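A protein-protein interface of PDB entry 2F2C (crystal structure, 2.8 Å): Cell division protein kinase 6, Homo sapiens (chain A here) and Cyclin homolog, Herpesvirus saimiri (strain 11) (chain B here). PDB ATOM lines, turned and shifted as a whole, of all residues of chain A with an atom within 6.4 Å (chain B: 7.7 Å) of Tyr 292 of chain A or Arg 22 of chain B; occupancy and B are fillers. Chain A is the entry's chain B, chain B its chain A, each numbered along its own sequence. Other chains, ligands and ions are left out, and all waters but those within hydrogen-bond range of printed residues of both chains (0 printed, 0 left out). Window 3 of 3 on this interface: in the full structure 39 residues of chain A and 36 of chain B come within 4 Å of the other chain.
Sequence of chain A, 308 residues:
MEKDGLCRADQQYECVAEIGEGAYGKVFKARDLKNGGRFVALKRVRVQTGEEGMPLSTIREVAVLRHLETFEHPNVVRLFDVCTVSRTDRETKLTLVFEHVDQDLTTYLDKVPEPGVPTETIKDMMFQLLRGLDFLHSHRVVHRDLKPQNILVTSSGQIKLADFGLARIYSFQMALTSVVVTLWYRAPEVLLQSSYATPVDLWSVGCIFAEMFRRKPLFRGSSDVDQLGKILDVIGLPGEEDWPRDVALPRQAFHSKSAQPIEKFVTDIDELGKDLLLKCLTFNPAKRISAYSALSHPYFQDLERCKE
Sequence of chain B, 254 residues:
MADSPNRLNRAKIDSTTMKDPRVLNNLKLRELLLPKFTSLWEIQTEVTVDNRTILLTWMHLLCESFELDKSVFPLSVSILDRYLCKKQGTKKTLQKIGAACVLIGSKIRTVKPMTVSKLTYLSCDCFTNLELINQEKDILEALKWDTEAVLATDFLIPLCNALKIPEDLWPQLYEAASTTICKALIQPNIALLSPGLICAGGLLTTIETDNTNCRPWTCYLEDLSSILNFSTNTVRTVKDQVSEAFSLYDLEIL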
ATOM      1  N   LEU A 130      -8.231 -19.950 -17.186  1.00  0.00           N
ATOM      2  CA  LEU A 130      -9.166 -21.069 -17.345  1.00  0.00           C
ATOM      3  C   LEU A 130      -9.742 -21.165 -18.753  1.00  0.00           C
ATOM      4  O   LEU A 130     -10.028 -22.265 -19.246  1.00  0.00           O
ATOM      5  CB  LEU A 130     -10.300 -20.977 -16.324  1.00  0.00           C
ATOM      6  CG  LEU A 130     -10.004 -21.516 -14.924  1.00  0.00           C
ATOM      7  CD1 LEU A 130     -11.127 -21.150 -13.937  1.00  0.00           C
ATOM      8  CD2 LEU A 130      -9.793 -23.032 -14.999  1.00  0.00           C
ATOM      9  N   ASP A 134      -9.561 -24.111 -21.330  1.00  0.00           N
ATOM     10  CA  ASP A 134     -10.785 -24.676 -21.873  1.00  0.00           C
ATOM     11  C   ASP A 134     -10.690 -24.837 -23.406  1.00  0.00           C
ATOM     12  O   ASP A 134     -11.176 -25.807 -23.997  1.00  0.00           O
ATOM     13  CB  ASP A 134     -11.954 -23.782 -21.486  1.00  0.00           C
ATOM     14  CG  ASP A 134     -13.243 -24.237 -22.086  1.00  0.00           C
ATOM     15  OD1 ASP A 134     -13.704 -25.338 -21.733  1.00  0.00           O
ATOM     16  OD2 ASP A 134     -13.864 -23.559 -22.928  1.00  0.00           O
ATOM     17  N   PHE A 135     -10.041 -23.869 -24.034  1.00  0.00           N
ATOM     18  CA  PHE A 135      -9.720 -23.929 -25.435  1.00  0.00           C
ATOM     19  C   PHE A 135      -8.903 -25.168 -25.764  1.00  0.00           C
ATOM     20  O   PHE A 135      -9.304 -26.006 -26.601  1.00  0.00           O
ATOM     21  CB  PHE A 135      -8.915 -22.697 -25.807  1.00  0.00           C
ATOM     22  CG  PHE A 135      -8.576 -22.618 -27.261  1.00  0.00           C
ATOM     23  CD1 PHE A 135      -9.586 -22.460 -28.216  1.00  0.00           C
ATOM     24  CD2 PHE A 135      -7.248 -22.700 -27.678  1.00  0.00           C
ATOM     25  CE1 PHE A 135      -9.279 -22.380 -29.572  1.00  0.00           C
ATOM     26  CE2 PHE A 135      -6.931 -22.618 -29.023  1.00  0.00           C
ATOM     27  CZ  PHE A 135      -7.949 -22.455 -29.975  1.00  0.00           C
ATOM     28  N   SER A 138     -10.451 -28.770 -25.296  1.00  0.00           N
ATOM     29  CA  SER A 138     -11.550 -29.036 -26.216  1.00  0.00           C
ATOM     30  C   SER A 138     -11.038 -29.364 -27.619  1.00  0.00           C
ATOM     31  O   SER A 138     -11.819 -29.741 -28.510  1.00  0.00           O
ATOM     32  CB  SER A 138     -12.499 -27.839 -26.265  1.00  0.00           C
ATOM     33  OG  SER A 138     -11.903 -26.757 -26.953  1.00  0.00           O
ATOM     34  N   LEU A 202      -5.524 -28.358 -14.266  1.00  0.00           N
ATOM     35  CA  LEU A 202      -6.274 -27.690 -13.221  1.00  0.00           C
ATOM     36  C   LEU A 202      -5.565 -27.732 -11.884  1.00  0.00           C
ATOM     37  O   LEU A 202      -5.727 -26.811 -11.078  1.00  0.00           O
ATOM     38  CB  LEU A 202      -7.686 -28.246 -13.120  1.00  0.00           C
ATOM     39  CG  LEU A 202      -8.479 -27.837 -14.368  1.00  0.00           C
ATOM     40  CD1 LEU A 202      -9.450 -28.916 -14.759  1.00  0.00           C
ATOM     41  CD2 LEU A 202      -9.150 -26.477 -14.225  1.00  0.00           C
ATOM     42  N   SER A 290     -13.282 -29.144 -13.901  1.00  0.00           N
ATOM     43  CA  SER A 290     -12.739 -28.972 -15.258  1.00  0.00           C
ATOM     44  C   SER A 290     -12.729 -27.495 -15.625  1.00  0.00           C
ATOM     45  O   SER A 290     -13.476 -26.709 -15.036  1.00  0.00           O
ATOM     46  CB  SER A 290     -13.550 -29.772 -16.267  1.00  0.00           C
ATOM     47  OG  SER A 290     -14.888 -29.299 -16.334  1.00  0.00           O
ATOM     48  N   ALA A 291     -11.888 -27.114 -16.582  1.00  0.00           N
ATOM     49  CA  ALA A 291     -11.822 -25.722 -17.059  1.00  0.00           C
ATOM     50  C   ALA A 291     -13.186 -25.150 -17.484  1.00  0.00           C
ATOM     51  O   ALA A 291     -13.563 -24.045 -17.076  1.00  0.00           O
ATOM     52  CB  ALA A 291     -10.815 -25.596 -18.196  1.00  0.00           C
ATOM     53  N   TYR A 292     -13.919 -25.906 -18.298  1.00  0.00           N
ATOM     54  CA  TYR A 292     -15.249 -25.488 -18.736  1.00  0.00           C
ATOM     55  C   TYR A 292     -16.190 -25.101 -17.573  1.00  0.00           C
ATOM     56  O   TYR A 292     -16.784 -24.013 -17.587  1.00  0.00           O
ATOM     57  CB  TYR A 292     -15.909 -26.557 -19.628  1.00  0.00           C
ATOM     58  CG  TYR A 292     -17.335 -26.223 -19.999  1.00  0.00           C
ATOM     59  CD1 TYR A 292     -17.620 -25.385 -21.088  1.00  0.00           C
ATOM     60  CD2 TYR A 292     -18.412 -26.719 -19.249  1.00  0.00           C
ATOM     61  CE1 TYR A 292     -18.940 -25.066 -21.440  1.00  0.00           C
ATOM     62  CE2 TYR A 292     -19.748 -26.391 -19.580  1.00  0.00           C
ATOM     63  CZ  TYR A 292     -20.001 -25.567 -20.680  1.00  0.00           C
ATOM     64  OH  TYR A 292     -21.306 -25.237 -21.010  1.00  0.00           O
ATOM     65  N   SER A 293     -16.349 -25.975 -16.582  1.00  0.00           N
ATOM     66  CA  SER A 293     -17.408 -25.737 -15.616  1.00  0.00           C
ATOM     67  C   SER A 293     -16.929 -24.847 -14.473  1.00  0.00           C
ATOM     68  O   SER A 293     -17.737 -24.161 -13.812  1.00  0.00           O
ATOM     69  CB  SER A 293     -18.033 -27.043 -15.138  1.00  0.00           C
ATOM     70  OG  SER A 293     -17.076 -27.824 -14.505  1.00  0.00           O
ATOM     71  N   ALA A 294     -15.614 -24.839 -14.272  1.00  0.00           N
ATOM     72  CA  ALA A 294     -14.964 -23.856 -13.409  1.00  0.00           C
ATOM     73  C   ALA A 294     -15.258 -22.435 -13.906  1.00  0.00           C
ATOM     74  O   ALA A 294     -15.560 -21.546 -13.121  1.00  0.00           O
ATOM     75  CB  ALA A 294     -13.456 -24.112 -13.343  1.00  0.00           C
ATOM     76  N   LEU A 295     -15.203 -22.234 -15.219  1.00  0.00           N
ATOM     77  CA  LEU A 295     -15.483 -20.920 -15.796  1.00  0.00           C
ATOM     78  C   LEU A 295     -16.869 -20.396 -15.412  1.00  0.00           C
ATOM     79  O   LEU A 295     -17.128 -19.198 -15.492  1.00  0.00           O
ATOM     80  CB  LEU A 295     -15.305 -20.932 -17.319  1.00  0.00           C
ATOM     81  CG  LEU A 295     -13.870 -20.894 -17.852  1.00  0.00           C
ATOM     82  CD1 LEU A 295     -13.856 -21.286 -19.320  1.00  0.00           C
ATOM     83  CD2 LEU A 295     -13.229 -19.531 -17.660  1.00  0.00           C
ATOM     84  N   SER A 296     -17.736 -21.307 -14.980  1.00  0.00           N
ATOM     85  CA  SER A 296     -19.103 -20.982 -14.589  1.00  0.00           C
ATOM     86  C   SER A 296     -19.346 -21.220 -13.091  1.00  0.00           C
ATOM     87  O   SER A 296     -20.484 -21.226 -12.627  1.00  0.00           O
ATOM     88  CB  SER A 296     -20.094 -21.783 -15.443  1.00  0.00           C
ATOM     89  OG  SER A 296     -19.719 -23.154 -15.462  1.00  0.00           O
ATOM     90  N   HIS A 297     -18.269 -21.424 -12.337  1.00  0.00           N
ATOM     91  CA  HIS A 297     -18.345 -21.420 -10.884  1.00  0.00           C
ATOM     92  C   HIS A 297     -18.723 -20.005 -10.419  1.00  0.00           C
ATOM     93  O   HIS A 297     -18.128 -19.033 -10.880  1.00  0.00           O
ATOM     94  CB  HIS A 297     -17.000 -21.851 -10.293  1.00  0.00           C
ATOM     95  CG  HIS A 297     -16.942 -21.803  -8.797  1.00  0.00           C
ATOM     96  ND1 HIS A 297     -16.869 -20.621  -8.090  1.00  0.00           N
ATOM     97  CD2 HIS A 297     -16.919 -22.792  -7.872  1.00  0.00           C
ATOM     98  CE1 HIS A 297     -16.819 -20.883  -6.797  1.00  0.00           C
ATOM     99  NE2 HIS A 297     -16.847 -22.193  -6.636  1.00  0.00           N
ATOM    100  N   THR B  16     -13.373 -34.863 -20.212  1.00  0.00           N
ATOM    101  CA  THR B  16     -13.089 -33.593 -20.866  1.00  0.00           C
ATOM    102  C   THR B  16     -12.687 -33.727 -22.342  1.00  0.00           C
ATOM    103  O   THR B  16     -13.022 -32.879 -23.170  1.00  0.00           O
ATOM    104  CB  THR B  16     -12.004 -32.869 -20.083  1.00  0.00           C
ATOM    105  OG1 THR B  16     -12.594 -32.236 -18.938  1.00  0.00           O
ATOM    106  CG2 THR B  16     -11.427 -31.715 -20.860  1.00  0.00           C
ATOM    107  N   LYS B  19     -15.771 -37.126 -23.833  1.00  0.00           N
ATOM    108  CA  LYS B  19     -17.214 -37.120 -23.682  1.00  0.00           C
ATOM    109  C   LYS B  19     -17.838 -35.777 -24.036  1.00  0.00           C
ATOM    110  O   LYS B  19     -19.061 -35.699 -24.247  1.00  0.00           O
ATOM    111  CB  LYS B  19     -17.598 -37.467 -22.242  1.00  0.00           C
ATOM    112  CG  LYS B  19     -17.507 -38.929 -21.875  1.00  0.00           C
ATOM    113  CD  LYS B  19     -17.750 -39.093 -20.364  1.00  0.00           C
ATOM    114  CE  LYS B  19     -18.459 -40.402 -20.045  1.00  0.00           C
ATOM    115  NZ  LYS B  19     -19.373 -40.812 -21.195  1.00  0.00           N
ATOM    116  N   ASP B  20     -17.023 -34.720 -24.073  1.00  0.00           N
ATOM    117  CA  ASP B  20     -17.531 -33.391 -24.420  1.00  0.00           C
ATOM    118  C   ASP B  20     -18.043 -33.339 -25.877  1.00  0.00           C
ATOM    119  O   ASP B  20     -17.278 -33.592 -26.819  1.00  0.00           O
ATOM    120  CB  ASP B  20     -16.482 -32.300 -24.159  1.00  0.00           C
ATOM    121  CG  ASP B  20     -17.055 -30.879 -24.303  1.00  0.00           C
ATOM    122  OD1 ASP B  20     -17.989 -30.683 -25.111  1.00  0.00           O
ATOM    123  OD2 ASP B  20     -16.632 -29.888 -23.660  1.00  0.00           O
ATOM    124  N   PRO B  21     -19.335 -33.036 -26.052  1.00  0.00           N
ATOM    125  CA  PRO B  21     -19.921 -32.955 -27.386  1.00  0.00           C
ATOM    126  C   PRO B  21     -19.107 -32.063 -28.295  1.00  0.00           C
ATOM    127  O   PRO B  21     -19.049 -32.323 -29.495  1.00  0.00           O
ATOM    128  CB  PRO B  21     -21.316 -32.353 -27.152  1.00  0.00           C
ATOM    129  CG  PRO B  21     -21.386 -31.999 -25.697  1.00  0.00           C
ATOM    130  CD  PRO B  21     -20.330 -32.773 -24.994  1.00  0.00           C
ATOM    131  N   ARG B  22     -18.442 -31.051 -27.747  1.00  0.00           N
ATOM    132  CA  ARG B  22     -17.784 -30.090 -28.632  1.00  0.00           C
ATOM    133  C   ARG B  22     -16.381 -30.445 -29.119  1.00  0.00           C
ATOM    134  O   ARG B  22     -15.895 -29.847 -30.084  1.00  0.00           O
ATOM    135  CB  ARG B  22     -17.930 -28.627 -28.164  1.00  0.00           C
ATOM    136  CG  ARG B  22     -17.302 -28.265 -26.878  1.00  0.00           C
ATOM    137  CD  ARG B  22     -17.961 -27.107 -26.175  1.00  0.00           C
ATOM    138  NE  ARG B  22     -17.310 -26.933 -24.869  1.00  0.00           N
ATOM    139  CZ  ARG B  22     -16.152 -26.301 -24.691  1.00  0.00           C
ATOM    140  NH1 ARG B  22     -15.522 -25.763 -25.731  1.00  0.00           N
ATOM    141  NH2 ARG B  22     -15.614 -26.214 -23.495  1.00  0.00           N
ATOM    142  N   VAL B  23     -15.772 -31.453 -28.500  1.00  0.00           N
ATOM    143  CA  VAL B  23     -14.545 -32.041 -29.002  1.00  0.00           C
ATOM    144  C   VAL B  23     -14.799 -32.631 -30.389  1.00  0.00           C
ATOM    145  O   VAL B  23     -13.993 -32.441 -31.295  1.00  0.00           O
ATOM    146  CB  VAL B  23     -13.972 -33.115 -27.996  1.00  0.00           C
ATOM    147  CG1 VAL B  23     -13.101 -34.194 -28.690  1.00  0.00           C
ATOM    148  CG2 VAL B  23     -13.218 -32.439 -26.828  1.00  0.00           C
ATOM    149  N   LEU B  24     -15.914 -33.339 -30.565  1.00  0.00           N
ATOM    150  CA  LEU B  24     -16.280 -33.893 -31.871  1.00  0.00           C
ATOM    151  C   LEU B  24     -16.466 -32.754 -32.866  1.00  0.00           C
ATOM    152  O   LEU B  24     -16.071 -32.846 -34.058  1.00  0.00           O
ATOM    153  CB  LEU B  24     -17.604 -34.637 -31.779  1.00  0.00           C
ATOM    154  CG  LEU B  24     -17.796 -35.933 -32.577  1.00  0.00           C
ATOM    155  CD1 LEU B  24     -19.273 -36.222 -32.748  1.00  0.00           C
ATOM    156  CD2 LEU B  24     -17.085 -35.951 -33.932  1.00  0.00           C
ATOM    157  N   ASN B  25     -17.098 -31.687 -32.361  1.00  0.00           N
ATOM    158  CA  ASN B  25     -17.402 -30.520 -33.158  1.00  0.00           C
ATOM    159  C   ASN B  25     -16.111 -29.942 -33.695  1.00  0.00           C
ATOM    160  O   ASN B  25     -16.037 -29.628 -34.893  1.00  0.00           O
ATOM    161  CB  ASN B  25     -18.108 -29.464 -32.312  1.00  0.00           C
ATOM    162  CG  ASN B  25     -19.589 -29.378 -32.593  1.00  0.00           C
ATOM    163  OD1 ASN B  25     -20.006 -29.005 -33.709  1.00  0.00           O
ATOM    164  ND2 ASN B  25     -20.404 -29.675 -31.573  1.00  0.00           N
ATOM    165  N   ASN B  26     -15.099 -29.826 -32.816  1.00  0.00           N
ATOM    166  CA  ASN B  26     -13.835 -29.203 -33.196  1.00  0.00           C
ATOM    167  C   ASN B  26     -13.015 -30.077 -34.131  1.00  0.00           C
ATOM    168  O   ASN B  26     -12.224 -29.574 -34.921  1.00  0.00           O
ATOM    169  CB  ASN B  26     -13.011 -28.807 -31.975  1.00  0.00           C
ATOM    170  CG  ASN B  26     -13.685 -27.742 -31.136  1.00  0.00           C
ATOM    171  OD1 ASN B  26     -14.002 -26.642 -31.616  1.00  0.00           O
ATOM    172  ND2 ASN B  26     -13.901 -28.055 -29.866  1.00  0.00           N
ATOM    173  N   LEU B  27     -13.206 -31.389 -34.036  1.00  0.00           N
ATOM    174  CA  LEU B  27     -12.488 -32.305 -34.881  1.00  0.00           C
ATOM    175  C   LEU B  27     -12.979 -32.146 -36.310  1.00  0.00           C
ATOM    176  O   LEU B  27     -12.168 -32.005 -37.235  1.00  0.00           O
ATOM    177  CB  LEU B  27     -12.647 -33.744 -34.394  1.00  0.00           C
ATOM    178  CG  LEU B  27     -11.619 -34.286 -33.399  1.00  0.00           C
ATOM    179  CD1 LEU B  27     -12.084 -35.638 -32.867  1.00  0.00           C
ATOM    180  CD2 LEU B  27     -10.211 -34.414 -34.013  1.00  0.00           C
ATOM    181  N   LYS B  28     -14.303 -32.129 -36.479  1.00  0.00           N
ATOM    182  CA  LYS B  28     -14.919 -31.823 -37.772  1.00  0.00           C
ATOM    183  C   LYS B  28     -14.452 -30.472 -38.305  1.00  0.00           C
ATOM    184  O   LYS B  28     -14.212 -30.325 -39.504  1.00  0.00           O
ATOM    185  CB  LYS B  28     -16.431 -31.769 -37.662  1.00  0.00           C
ATOM    186  CG  LYS B  28     -17.140 -33.059 -37.347  1.00  0.00           C
ATOM    187  CD  LYS B  28     -18.483 -32.631 -36.809  1.00  0.00           C
ATOM    188  CE  LYS B  28     -19.585 -33.611 -37.009  1.00  0.00           C
ATOM    189  NZ  LYS B  28     -20.843 -32.835 -37.344  1.00  0.00           N
ATOM    190  N   LEU B  29     -14.344 -29.477 -37.434  1.00  0.00           N
ATOM    191  CA  LEU B  29     -13.954 -28.137 -37.870  1.00  0.00           C
ATOM    192  C   LEU B  29     -12.513 -28.108 -38.342  1.00  0.00           C
ATOM    193  O   LEU B  29     -12.238 -27.648 -39.443  1.00  0.00           O
ATOM    194  CB  LEU B  29     -14.145 -27.132 -36.738  1.00  0.00           C
ATOM    195  CG  LEU B  29     -15.082 -25.955 -37.015  1.00  0.00           C
ATOM    196  CD1 LEU B  29     -15.494 -25.271 -35.715  1.00  0.00           C
ATOM    197  CD2 LEU B  29     -14.458 -24.964 -38.009  1.00  0.00           C
ATOM    198  N   ARG B  30     -11.600 -28.629 -37.519  1.00  0.00           N
ATOM    199  CA  ARG B  30     -10.168 -28.665 -37.848  1.00  0.00           C
ATOM    200  C   ARG B  30      -9.889 -29.621 -39.015  1.00  0.00           C
ATOM    201  O   ARG B  30      -8.910 -29.459 -39.762  1.00  0.00           O
ATOM    202  CB  ARG B  30      -9.308 -28.992 -36.624  1.00  0.00           C
ATOM    203  CG  ARG B  30      -9.461 -28.001 -35.435  1.00  0.00           C
ATOM    204  CD  ARG B  30      -8.481 -28.213 -34.275  1.00  0.00           C
ATOM    205  NE  ARG B  30      -8.169 -29.628 -34.126  1.00  0.00           N
ATOM    206  CZ  ARG B  30      -8.736 -30.450 -33.264  1.00  0.00           C
ATOM    207  NH1 ARG B  30      -9.636 -30.015 -32.406  1.00  0.00           N
ATOM    208  NH2 ARG B  30      -8.386 -31.718 -33.252  1.00  0.00           N
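The backbone carbonyl oxygen (O) of Ser 138 of chain A sits at hydrogen-bond distance from the side-chain amide nitrogen (ND2) of Asn 26 of chain B (3.0 Å). The guanidinium group (NH2) of Arg 22 of chain B is in salt-bridge range of the side-chain carboxylate (OD1) of Asp 134 of chain A (2.7 Å).
OG of Ser 138 of chain A sits at hydrogen-bond distance from O of Asp 134 of chain A, at 3.2 Å. OG of Ser 290 of chain A sits at hydrogen-bond distance from OG of Ser 293 of chain A, at 3.2 Å. The backbone carbonyl oxygen of Phe 135 of chain A is in hydrogen-bond range of the side-chain hydroxyl of Ser 138 of chain A (2.7 Å). OD1 of Asp 134 of chain A lies close to N of Tyr 292 of chain A (3.5 Å). The guanidinium group (NE) of Arg 22 of chain B is in salt-bridge range of the side-chain carboxylate (OD2) of Asp 20 of chain B. The backbone carbonyl oxygen (O) of Arg 22 of chain B lies within hydrogen-bond range of the side-chain amide nitrogen (ND2) of Asn 26 of chain B, at 2.7 Å.
Among the printed residues, pairs that only touch across the chains: Ser 138 of chain A with Arg 22 of chain B (3.7 Å), Ser 138 of chain A with Val 23 of chain B (3.5 Å), Ser 290 of chain A with Thr 16 of chain B (3.8 Å) and Tyr 292 of chain A with Arg 22 of chain B (3.2 Å).
Of the printed residues of chain B, Asp 134 of chain A touches Arg 22 (2.7 Å). Of the printed residues of chain B, Ser 138 of chain A touches Arg 22 (3.7 Å), Val 23 (3.5 Å) and Asn 26 (3.0 Å). Printed residues of chain B within 4 Å of Ser 290 of chain A: Thr 16. No residue of chain B comes within 4 Å of Ala 291 of chain A. Tyr 292 of chain A touches one residue of chain B. Of the printed residues of chain A, Thr 16 of chain B touches Ser 290. Of chain A, only Asp 134 (2.7 Å), Ser 138 (3.7 Å) and Tyr 292 (3.2 Å) come within 4 Å of Arg 22 of chain B. Printed residues of chain A within 4 Å of Asn 26 of chain B: Ser 138. The nearest residue of chain B that does not touch Tyr 292 of chain A is Asp 20 of chain B (5.2 Å).
Of the 13 printed residues of chain B, 4 touch a printed residue of chain A. Of the 13 printed residues of chain A, 4 touch a printed residue of chain B. Hydrophobic or aromatic side chains of chain A within 4 Å of the printed part of chain B: Tyr 292. Among the printed residues, 6 pairs touch across the chains. Among the printed residues, Asp or Glu carboxylates within 4 Å of a Lys or Arg side-chain nitrogen of the other chain: Asp 134 of chain A with Arg 22 of chain B (2.7 Å).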
